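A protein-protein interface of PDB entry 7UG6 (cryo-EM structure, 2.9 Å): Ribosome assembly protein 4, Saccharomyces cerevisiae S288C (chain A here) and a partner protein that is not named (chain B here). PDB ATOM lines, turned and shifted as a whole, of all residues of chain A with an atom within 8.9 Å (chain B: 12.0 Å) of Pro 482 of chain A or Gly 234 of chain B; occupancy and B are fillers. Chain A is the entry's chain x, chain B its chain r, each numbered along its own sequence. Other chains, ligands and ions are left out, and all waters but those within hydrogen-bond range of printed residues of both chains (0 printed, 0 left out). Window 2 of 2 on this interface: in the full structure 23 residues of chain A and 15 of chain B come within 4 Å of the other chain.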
ATOM      1  N   THR A 132     -32.397   3.028  -8.977  1.00  0.00           N
ATOM      2  CA  THR A 132     -31.446   2.492  -9.948  1.00  0.00           C
ATOM      3  C   THR A 132     -31.154   3.364 -11.163  1.00  0.00           C
ATOM      4  O   THR A 132     -30.084   3.200 -11.752  1.00  0.00           O
ATOM      5  CB  THR A 132     -31.912   1.123 -10.462  1.00  0.00           C
ATOM      6  OG1 THR A 132     -32.971   1.304 -11.402  1.00  0.00           O
ATOM      7  CG2 THR A 132     -32.401   0.245  -9.341  1.00  0.00           C
ATOM      8  N   ARG A 133     -32.046   4.244 -11.591  1.00  0.00           N
ATOM      9  CA  ARG A 133     -31.871   4.922 -12.867  1.00  0.00           C
ATOM     10  C   ARG A 133     -31.788   6.424 -12.687  1.00  0.00           C
ATOM     11  O   ARG A 133     -32.680   7.032 -12.096  1.00  0.00           O
ATOM     12  CB  ARG A 133     -33.031   4.641 -13.811  1.00  0.00           C
ATOM     13  CG  ARG A 133     -33.533   3.235 -13.804  1.00  0.00           C
ATOM     14  CD  ARG A 133     -34.717   3.110 -14.716  1.00  0.00           C
ATOM     15  NE  ARG A 133     -35.731   4.106 -14.409  1.00  0.00           N
ATOM     16  CZ  ARG A 133     -36.015   5.140 -15.188  1.00  0.00           C
ATOM     17  NH1 ARG A 133     -35.346   5.325 -16.314  1.00  0.00           N
ATOM     18  NH2 ARG A 133     -36.956   5.999 -14.836  1.00  0.00           N
ATOM     19  N   SER A 134     -30.750   7.027 -13.250  1.00  0.00           N
ATOM     20  CA  SER A 134     -30.698   8.479 -13.336  1.00  0.00           C
ATOM     21  C   SER A 134     -31.744   8.903 -14.341  1.00  0.00           C
ATOM     22  O   SER A 134     -31.593   8.653 -15.540  1.00  0.00           O
ATOM     23  CB  SER A 134     -29.319   8.969 -13.757  1.00  0.00           C
ATOM     24  OG  SER A 134     -29.339  10.366 -13.996  1.00  0.00           O
ATOM     25  N   SER A 135     -32.815   9.522 -13.851  1.00  0.00           N
ATOM     26  CA  SER A 135     -33.883   9.965 -14.733  1.00  0.00           C
ATOM     27  C   SER A 135     -33.338  10.888 -15.813  1.00  0.00           C
ATOM     28  O   SER A 135     -33.365  10.553 -17.002  1.00  0.00           O
ATOM     29  CB  SER A 135     -34.968  10.649 -13.916  1.00  0.00           C
ATOM     30  OG  SER A 135     -35.844   9.694 -13.348  1.00  0.00           O
ATOM     31  N   HIS A 442     -16.680   2.910  -2.506  1.00  0.00           N
ATOM     32  CA  HIS A 442     -16.317   4.253  -2.903  1.00  0.00           C
ATOM     33  C   HIS A 442     -14.805   4.364  -3.000  1.00  0.00           C
ATOM     34  O   HIS A 442     -14.071   3.767  -2.214  1.00  0.00           O
ATOM     35  CB  HIS A 442     -16.853   5.267  -1.902  1.00  0.00           C
ATOM     36  CG  HIS A 442     -18.284   5.626  -2.115  1.00  0.00           C
ATOM     37  ND1 HIS A 442     -18.724   6.292  -3.235  1.00  0.00           N
ATOM     38  CD2 HIS A 442     -19.375   5.426  -1.343  1.00  0.00           C
ATOM     39  CE1 HIS A 442     -20.026   6.485  -3.148  1.00  0.00           C
ATOM     40  NE2 HIS A 442     -20.448   5.962  -2.012  1.00  0.00           N
ATOM     41  N   ASP A 464     -15.721  10.924  -5.456  1.00  0.00           N
ATOM     42  CA  ASP A 464     -15.799  10.431  -6.810  1.00  0.00           C
ATOM     43  C   ASP A 464     -17.164  10.802  -7.369  1.00  0.00           C
ATOM     44  O   ASP A 464     -18.009  11.382  -6.688  1.00  0.00           O
ATOM     45  CB  ASP A 464     -15.499   8.928  -6.887  1.00  0.00           C
ATOM     46  CG  ASP A 464     -16.504   8.057  -6.158  1.00  0.00           C
ATOM     47  OD1 ASP A 464     -17.708   8.350  -6.136  1.00  0.00           O
ATOM     48  OD2 ASP A 464     -16.080   7.029  -5.602  1.00  0.00           O
ATOM     49  N   THR A 465     -17.387  10.469  -8.608  1.00  0.00           N
ATOM     50  CA  THR A 465     -18.581  10.968  -9.238  1.00  0.00           C
ATOM     51  C   THR A 465     -19.835  10.213  -8.832  1.00  0.00           C
ATOM     52  O   THR A 465     -20.931  10.638  -9.187  1.00  0.00           O
ATOM     53  CB  THR A 465     -18.388  10.912 -10.745  1.00  0.00           C
ATOM     54  OG1 THR A 465     -17.890   9.619 -11.101  1.00  0.00           O
ATOM     55  CG2 THR A 465     -17.368  11.941 -11.155  1.00  0.00           C
ATOM     56  N   THR A 466     -19.723   9.134  -8.070  1.00  0.00           N
ATOM     57  CA  THR A 466     -20.757   8.113  -8.028  1.00  0.00           C
ATOM     58  C   THR A 466     -21.617   8.204  -6.780  1.00  0.00           C
ATOM     59  O   THR A 466     -21.129   8.455  -5.680  1.00  0.00           O
ATOM     60  CB  THR A 466     -20.148   6.713  -8.091  1.00  0.00           C
ATOM     61  OG1 THR A 466     -19.312   6.508  -6.951  1.00  0.00           O
ATOM     62  CG2 THR A 466     -19.327   6.548  -9.332  1.00  0.00           C
ATOM     63  N   LEU A 467     -22.908   7.979  -6.971  1.00  0.00           N
ATOM     64  CA  LEU A 467     -23.815   7.610  -5.900  1.00  0.00           C
ATOM     65  C   LEU A 467     -23.836   6.100  -5.799  1.00  0.00           C
ATOM     66  O   LEU A 467     -23.583   5.401  -6.779  1.00  0.00           O
ATOM     67  CB  LEU A 467     -25.238   8.102  -6.156  1.00  0.00           C
ATOM     68  CG  LEU A 467     -25.631   9.553  -5.942  1.00  0.00           C
ATOM     69  CD1 LEU A 467     -25.075  10.410  -7.036  1.00  0.00           C
ATOM     70  CD2 LEU A 467     -27.126   9.628  -5.933  1.00  0.00           C
ATOM     71  N   LYS A 468     -24.142   5.597  -4.616  1.00  0.00           N
ATOM     72  CA  LYS A 468     -24.254   4.166  -4.401  1.00  0.00           C
ATOM     73  C   LYS A 468     -25.349   3.918  -3.383  1.00  0.00           C
ATOM     74  O   LYS A 468     -25.583   4.759  -2.515  1.00  0.00           O
ATOM     75  CB  LYS A 468     -22.934   3.586  -3.916  1.00  0.00           C
ATOM     76  CG  LYS A 468     -21.887   3.487  -4.984  1.00  0.00           C
ATOM     77  CD  LYS A 468     -20.560   3.108  -4.429  1.00  0.00           C
ATOM     78  CE  LYS A 468     -19.611   2.819  -5.536  1.00  0.00           C
ATOM     79  NZ  LYS A 468     -19.425   4.005  -6.387  1.00  0.00           N
ATOM     80  N   VAL A 469     -26.035   2.784  -3.488  1.00  0.00           N
ATOM     81  CA  VAL A 469     -27.033   2.433  -2.492  1.00  0.00           C
ATOM     82  C   VAL A 469     -26.617   1.113  -1.874  1.00  0.00           C
ATOM     83  O   VAL A 469     -25.963   0.282  -2.507  1.00  0.00           O
ATOM     84  CB  VAL A 469     -28.465   2.327  -3.049  1.00  0.00           C
ATOM     85  CG1 VAL A 469     -28.923   3.645  -3.629  1.00  0.00           C
ATOM     86  CG2 VAL A 469     -28.580   1.231  -4.000  1.00  0.00           C
ATOM     87  N   VAL A 479     -26.629  -1.114  -5.860  1.00  0.00           N
ATOM     88  CA  VAL A 479     -26.326  -0.637  -7.205  1.00  0.00           C
ATOM     89  C   VAL A 479     -25.361   0.534  -7.117  1.00  0.00           C
ATOM     90  O   VAL A 479     -25.502   1.408  -6.259  1.00  0.00           O
ATOM     91  CB  VAL A 479     -27.596  -0.260  -8.001  1.00  0.00           C
ATOM     92  CG1 VAL A 479     -28.322   0.865  -7.386  1.00  0.00           C
ATOM     93  CG2 VAL A 479     -27.230   0.139  -9.406  1.00  0.00           C
ATOM     94  N   ASP A 480     -24.346   0.520  -7.974  1.00  0.00           N
ATOM     95  CA  ASP A 480     -23.533   1.695  -8.208  1.00  0.00           C
ATOM     96  C   ASP A 480     -24.236   2.595  -9.204  1.00  0.00           C
ATOM     97  O   ASP A 480     -24.824   2.129 -10.179  1.00  0.00           O
ATOM     98  CB  ASP A 480     -22.160   1.313  -8.746  1.00  0.00           C
ATOM     99  CG  ASP A 480     -21.246   2.514  -8.912  1.00  0.00           C
ATOM    100  OD1 ASP A 480     -20.214   2.387  -9.603  1.00  0.00           O
ATOM    101  OD2 ASP A 480     -21.555   3.586  -8.349  1.00  0.00           O
ATOM    102  N   LEU A 481     -24.171   3.895  -8.958  1.00  0.00           N
ATOM    103  CA  LEU A 481     -24.955   4.872  -9.711  1.00  0.00           C
ATOM    104  C   LEU A 481     -24.051   5.968 -10.241  1.00  0.00           C
ATOM    105  O   LEU A 481     -24.018   7.083  -9.714  1.00  0.00           O
ATOM    106  CB  LEU A 481     -26.068   5.456  -8.846  1.00  0.00           C
ATOM    107  CG  LEU A 481     -27.127   4.462  -8.395  1.00  0.00           C
ATOM    108  CD1 LEU A 481     -28.134   5.121  -7.496  1.00  0.00           C
ATOM    109  CD2 LEU A 481     -27.802   3.902  -9.597  1.00  0.00           C
ATOM    110  N   PRO A 482     -23.316   5.694 -11.298  1.00  0.00           N
ATOM    111  CA  PRO A 482     -22.528   6.732 -11.953  1.00  0.00           C
ATOM    112  C   PRO A 482     -23.444   7.621 -12.776  1.00  0.00           C
ATOM    113  O   PRO A 482     -24.625   7.347 -12.943  1.00  0.00           O
ATOM    114  CB  PRO A 482     -21.596   5.930 -12.842  1.00  0.00           C
ATOM    115  CG  PRO A 482     -22.422   4.767 -13.223  1.00  0.00           C
ATOM    116  CD  PRO A 482     -23.234   4.420 -12.020  1.00  0.00           C
ATOM    117  N   GLY A 483     -22.872   8.681 -13.322  1.00  0.00           N
ATOM    118  CA  GLY A 483     -23.655   9.563 -14.155  1.00  0.00           C
ATOM    119  C   GLY A 483     -23.331  11.024 -13.966  1.00  0.00           C
ATOM    120  O   GLY A 483     -23.483  11.818 -14.894  1.00  0.00           O
ATOM    121  N   HIS A 484     -22.892  11.400 -12.775  1.00  0.00           N
ATOM    122  CA  HIS A 484     -22.408  12.753 -12.567  1.00  0.00           C
ATOM    123  C   HIS A 484     -21.050  12.923 -13.216  1.00  0.00           C
ATOM    124  O   HIS A 484     -20.189  12.053 -13.097  1.00  0.00           O
ATOM    125  CB  HIS A 484     -22.306  13.057 -11.083  1.00  0.00           C
ATOM    126  CG  HIS A 484     -23.570  13.577 -10.485  1.00  0.00           C
ATOM    127  ND1 HIS A 484     -23.916  14.908 -10.535  1.00  0.00           N
ATOM    128  CD2 HIS A 484     -24.557  12.954  -9.808  1.00  0.00           C
ATOM    129  CE1 HIS A 484     -25.068  15.080  -9.919  1.00  0.00           C
ATOM    130  NE2 HIS A 484     -25.477  13.910  -9.467  1.00  0.00           N
ATOM    131  N   LYS A 485     -20.852  14.038 -13.906  1.00  0.00           N
ATOM    132  CA  LYS A 485     -19.524  14.306 -14.425  1.00  0.00           C
ATOM    133  C   LYS A 485     -18.515  14.540 -13.314  1.00  0.00           C
ATOM    134  O   LYS A 485     -17.351  14.161 -13.467  1.00  0.00           O
ATOM    135  CB  LYS A 485     -19.544  15.515 -15.368  1.00  0.00           C
ATOM    136  CG  LYS A 485     -18.206  15.802 -16.057  1.00  0.00           C
ATOM    137  CD  LYS A 485     -17.376  16.844 -15.298  1.00  0.00           C
ATOM    138  CE  LYS A 485     -15.991  17.003 -15.884  1.00  0.00           C
ATOM    139  NZ  LYS A 485     -15.152  17.879 -15.032  1.00  0.00           N
ATOM    140  N   ASP A 486     -18.927  15.151 -12.211  1.00  0.00           N
ATOM    141  CA  ASP A 486     -17.987  15.592 -11.200  1.00  0.00           C
ATOM    142  C   ASP A 486     -18.512  15.189  -9.831  1.00  0.00           C
ATOM    143  O   ASP A 486     -19.570  14.571  -9.710  1.00  0.00           O
ATOM    144  CB  ASP A 486     -17.758  17.101 -11.315  1.00  0.00           C
ATOM    145  CG  ASP A 486     -16.400  17.513 -10.821  1.00  0.00           C
ATOM    146  OD1 ASP A 486     -15.812  16.758 -10.024  1.00  0.00           O
ATOM    147  OD2 ASP A 486     -15.917  18.582 -11.238  1.00  0.00           O
ATOM    148  N   VAL A 488     -19.997  14.853  -6.069  1.00  0.00           N
ATOM    149  CA  VAL A 488     -21.369  15.064  -5.631  1.00  0.00           C
ATOM    150  C   VAL A 488     -21.379  15.418  -4.155  1.00  0.00           C
ATOM    151  O   VAL A 488     -20.797  14.712  -3.325  1.00  0.00           O
ATOM    152  CB  VAL A 488     -22.237  13.836  -5.927  1.00  0.00           C
ATOM    153  CG1 VAL A 488     -22.407  13.728  -7.375  1.00  0.00           C
ATOM    154  CG2 VAL A 488     -21.521  12.608  -5.512  1.00  0.00           C
ATOM    155  N   SER A 502     -29.377  14.271  -6.304  1.00  0.00           N
ATOM    156  CA  SER A 502     -27.962  14.472  -6.106  1.00  0.00           C
ATOM    157  C   SER A 502     -27.591  15.811  -6.690  1.00  0.00           C
ATOM    158  O   SER A 502     -28.357  16.422  -7.432  1.00  0.00           O
ATOM    159  CB  SER A 502     -27.148  13.360  -6.742  1.00  0.00           C
ATOM    160  OG  SER A 502     -27.250  13.430  -8.138  1.00  0.00           O
ATOM    161  N   ASP A 506     -20.901  19.274 -10.692  1.00  0.00           N
ATOM    162  CA  ASP A 506     -21.373  19.113 -12.060  1.00  0.00           C
ATOM    163  C   ASP A 506     -22.353  20.193 -12.485  1.00  0.00           C
ATOM    164  O   ASP A 506     -22.619  20.312 -13.685  1.00  0.00           O
ATOM    165  CB  ASP A 506     -22.022  17.742 -12.209  1.00  0.00           C
ATOM    166  CG  ASP A 506     -21.994  17.236 -13.627  1.00  0.00           C
ATOM    167  OD1 ASP A 506     -21.462  17.942 -14.507  1.00  0.00           O
ATOM    168  OD2 ASP A 506     -22.484  16.115 -13.866  1.00  0.00           O
ATOM    169  N   ARG A 510     -29.359  15.726 -10.640  1.00  0.00           N
ATOM    170  CA  ARG A 510     -29.796  14.410 -11.069  1.00  0.00           C
ATOM    171  C   ARG A 510     -30.959  13.985 -10.194  1.00  0.00           C
ATOM    172  O   ARG A 510     -30.935  14.199  -8.982  1.00  0.00           O
ATOM    173  CB  ARG A 510     -28.681  13.373 -10.968  1.00  0.00           C
ATOM    174  CG  ARG A 510     -27.548  13.543 -11.918  1.00  0.00           C
ATOM    175  CD  ARG A 510     -28.044  13.370 -13.307  1.00  0.00           C
ATOM    176  NE  ARG A 510     -26.982  13.474 -14.290  1.00  0.00           N
ATOM    177  CZ  ARG A 510     -26.562  12.452 -15.010  1.00  0.00           C
ATOM    178  NH1 ARG A 510     -27.145  11.278 -14.859  1.00  0.00           N
ATOM    179  NH2 ARG A 510     -25.590  12.609 -15.893  1.00  0.00           N
ATOM    180  N   TRP A 512     -33.048  10.411  -9.424  1.00  0.00           N
ATOM    181  CA  TRP A 512     -32.901   8.988  -9.640  1.00  0.00           C
ATOM    182  C   TRP A 512     -34.133   8.304  -9.091  1.00  0.00           C
ATOM    183  O   TRP A 512     -34.735   8.783  -8.133  1.00  0.00           O
ATOM    184  CB  TRP A 512     -31.650   8.435  -8.965  1.00  0.00           C
ATOM    185  CG  TRP A 512     -30.412   9.226  -9.163  1.00  0.00           C
ATOM    186  CD1 TRP A 512     -30.154  10.470  -8.690  1.00  0.00           C
ATOM    187  CD2 TRP A 512     -29.239   8.810  -9.852  1.00  0.00           C
ATOM    188  NE1 TRP A 512     -28.902  10.863  -9.056  1.00  0.00           N
ATOM    189  CE2 TRP A 512     -28.319   9.860  -9.776  1.00  0.00           C
ATOM    190  CE3 TRP A 512     -28.880   7.651 -10.530  1.00  0.00           C
ATOM    191  CZ2 TRP A 512     -27.075   9.792 -10.354  1.00  0.00           C
ATOM    192  CZ3 TRP A 512     -27.648   7.587 -11.106  1.00  0.00           C
ATOM    193  CH2 TRP A 512     -26.758   8.649 -11.017  1.00  0.00           C
ATOM    194  N   GLY B 229      -8.906   7.839  -7.223  1.00  0.00           N
ATOM    195  CA  GLY B 229     -10.345   7.677  -7.270  1.00  0.00           C
ATOM    196  C   GLY B 229     -11.020   8.172  -8.526  1.00  0.00           C
ATOM    197  O   GLY B 229     -12.101   8.761  -8.447  1.00  0.00           O
ATOM    198  N   MET B 230     -10.418   7.949  -9.686  1.00  0.00           N
ATOM    199  CA  MET B 230     -11.052   8.313 -10.940  1.00  0.00           C
ATOM    200  C   MET B 230     -12.006   7.211 -11.366  1.00  0.00           C
ATOM    201  O   MET B 230     -11.638   6.038 -11.409  1.00  0.00           O
ATOM    202  CB  MET B 230     -10.020   8.559 -12.037  1.00  0.00           C
ATOM    203  CG  MET B 230      -9.150   9.760 -11.795  1.00  0.00           C
ATOM    204  SD  MET B 230      -7.998  10.065 -13.134  1.00  0.00           S
ATOM    205  CE  MET B 230      -6.832   8.762 -12.850  1.00  0.00           C
ATOM    206  N   VAL B 231     -13.235   7.598 -11.675  1.00  0.00           N
ATOM    207  CA  VAL B 231     -14.273   6.671 -12.088  1.00  0.00           C
ATOM    208  C   VAL B 231     -14.764   7.098 -13.456  1.00  0.00           C
ATOM    209  O   VAL B 231     -15.099   8.268 -13.660  1.00  0.00           O
ATOM    210  CB  VAL B 231     -15.439   6.639 -11.090  1.00  0.00           C
ATOM    211  CG1 VAL B 231     -16.551   5.801 -11.626  1.00  0.00           C
ATOM    212  CG2 VAL B 231     -14.976   6.100  -9.786  1.00  0.00           C
ATOM    213  N   THR B 232     -14.805   6.160 -14.389  1.00  0.00           N
ATOM    214  CA  THR B 232     -15.317   6.468 -15.707  1.00  0.00           C
ATOM    215  C   THR B 232     -16.833   6.333 -15.721  1.00  0.00           C
ATOM    216  O   THR B 232     -17.431   5.675 -14.869  1.00  0.00           O
ATOM    217  CB  THR B 232     -14.690   5.552 -16.747  1.00  0.00           C
ATOM    218  OG1 THR B 232     -15.151   5.924 -18.052  1.00  0.00           O
ATOM    219  CG2 THR B 232     -15.064   4.121 -16.478  1.00  0.00           C
ATOM    220  N   ALA B 233     -17.461   6.994 -16.689  1.00  0.00           N
ATOM    221  CA  ALA B 233     -18.891   6.823 -16.880  1.00  0.00           C
ATOM    222  C   ALA B 233     -19.179   5.367 -17.193  1.00  0.00           C
ATOM    223  O   ALA B 233     -18.468   4.737 -17.979  1.00  0.00           O
ATOM    224  CB  ALA B 233     -19.389   7.721 -18.003  1.00  0.00           C
ATOM    225  N   GLY B 234     -20.206   4.827 -16.571  1.00  0.00           N
ATOM    226  CA  GLY B 234     -20.441   3.405 -16.612  1.00  0.00           C
ATOM    227  C   GLY B 234     -20.035   2.690 -15.348  1.00  0.00           C
ATOM    228  O   GLY B 234     -20.305   1.492 -15.221  1.00  0.00           O
ATOM    229  N   GLY B 235     -19.386   3.375 -14.420  1.00  0.00           N
ATOM    230  CA  GLY B 235     -19.210   2.885 -13.080  1.00  0.00           C
ATOM    231  C   GLY B 235     -17.919   2.146 -12.833  1.00  0.00           C
ATOM    232  O   GLY B 235     -17.593   1.881 -11.674  1.00  0.00           O
ATOM    233  N   LYS B 236     -17.190   1.791 -13.878  1.00  0.00           N
ATOM    234  CA  LYS B 236     -15.879   1.198 -13.690  1.00  0.00           C
ATOM    235  C   LYS B 236     -14.948   2.231 -13.081  1.00  0.00           C
ATOM    236  O   LYS B 236     -15.069   3.425 -13.357  1.00  0.00           O
ATOM    237  CB  LYS B 236     -15.328   0.708 -15.021  1.00  0.00           C
ATOM    238  CG  LYS B 236     -16.279  -0.170 -15.792  1.00  0.00           C
ATOM    239  CD  LYS B 236     -16.342  -1.553 -15.193  1.00  0.00           C
ATOM    240  CE  LYS B 236     -17.289  -2.427 -15.964  1.00  0.00           C
ATOM    241  NZ  LYS B 236     -18.517  -1.674 -16.327  1.00  0.00           N
ATOM    242  N   VAL B 237     -14.030   1.789 -12.238  1.00  0.00           N
ATOM    243  CA  VAL B 237     -13.094   2.716 -11.622  1.00  0.00           C
ATOM    244  C   VAL B 237     -11.745   2.550 -12.305  1.00  0.00           C
ATOM    245  O   VAL B 237     -11.309   1.434 -12.598  1.00  0.00           O
ATOM    246  CB  VAL B 237     -13.002   2.531 -10.092  1.00  0.00           C
ATOM    247  CG1 VAL B 237     -14.373   2.566  -9.479  1.00  0.00           C
ATOM    248  CG2 VAL B 237     -12.333   1.301  -9.705  1.00  0.00           C
ATOM    249  N   VAL B 238     -11.119   3.665 -12.621  1.00  0.00           N
ATOM    250  CA  VAL B 238      -9.853   3.671 -13.332  1.00  0.00           C
ATOM    251  C   VAL B 238      -8.741   3.444 -12.328  1.00  0.00           C
ATOM    252  O   VAL B 238      -8.593   4.211 -11.372  1.00  0.00           O
ATOM    253  CB  VAL B 238      -9.653   4.998 -14.072  1.00  0.00           C
ATOM    254  CG1 VAL B 238      -8.408   4.959 -14.907  1.00  0.00           C
ATOM    255  CG2 VAL B 238     -10.853   5.304 -14.924  1.00  0.00           C
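O of Gly 235 of chain B lies close to OD1 of Asp 480 of chain A.
The side-chain amino group (NZ) of Lys 468 of chain A sits at hydrogen-bond distance from the side-chain hydroxyl (OG1) of Thr 466 of chain A (2.6 Å).
The side-chain hydroxyl of Thr 466 of chain A sits at hydrogen-bond distance from the side-chain carboxylate of Asp 464 of chain A, at 2.6 Å.
NZ of Lys 468 of chain A is in salt-bridge range of OD2 of Asp 480 of chain A (2.9 Å).
Among the printed residues, pairs that only touch across the chains: Asp 464 of chain A with Gly 229 of chain B, Thr 465 of chain A with Val 231 of chain B, Thr 466 of chain A with Val 231 of chain B, Pro 482 of chain A with Gly 234 of chain B and Pro 482 of chain A with Gly 235 of chain B.
Pro 482 of chain A touches just these residues of chain B: Gly 234 (3.8 Å) and Gly 235 (3.5 Å).
Gly 234 of chain B touches one residue of chain A.
No residue of chain B comes within 4 Å of Ser 134 of chain A.
Of chain B, only Val 231 comes within 4 Å of Thr 465 of chain A.
Printed residues of chain B within 4 Å of Asp 480 of chain A: Gly 235.
Ala 233 of chain B touches none of the printed residues of chain A.
Printed residues of chain A within 4 Å of Val 231 of chain B: Thr 465 (3.9 Å) and Thr 466 (3.7 Å).
Of the printed residues of chain B, Asp 464 of chain A touches Gly 229.
The nearest printed residue of chain A that does not touch Gly 234 of chain B is Asp 480 of chain A (5.7 Å).
Hydrophobic or aromatic side chains of chain B within 4 Å of the printed part of chain A: Val 231.
Among the printed residues, 6 pairs touch across the chains.
Among the printed residues, no Asp or Glu carboxylate lies within 4 Å of a Lys or Arg side-chain nitrogen of the other chain.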
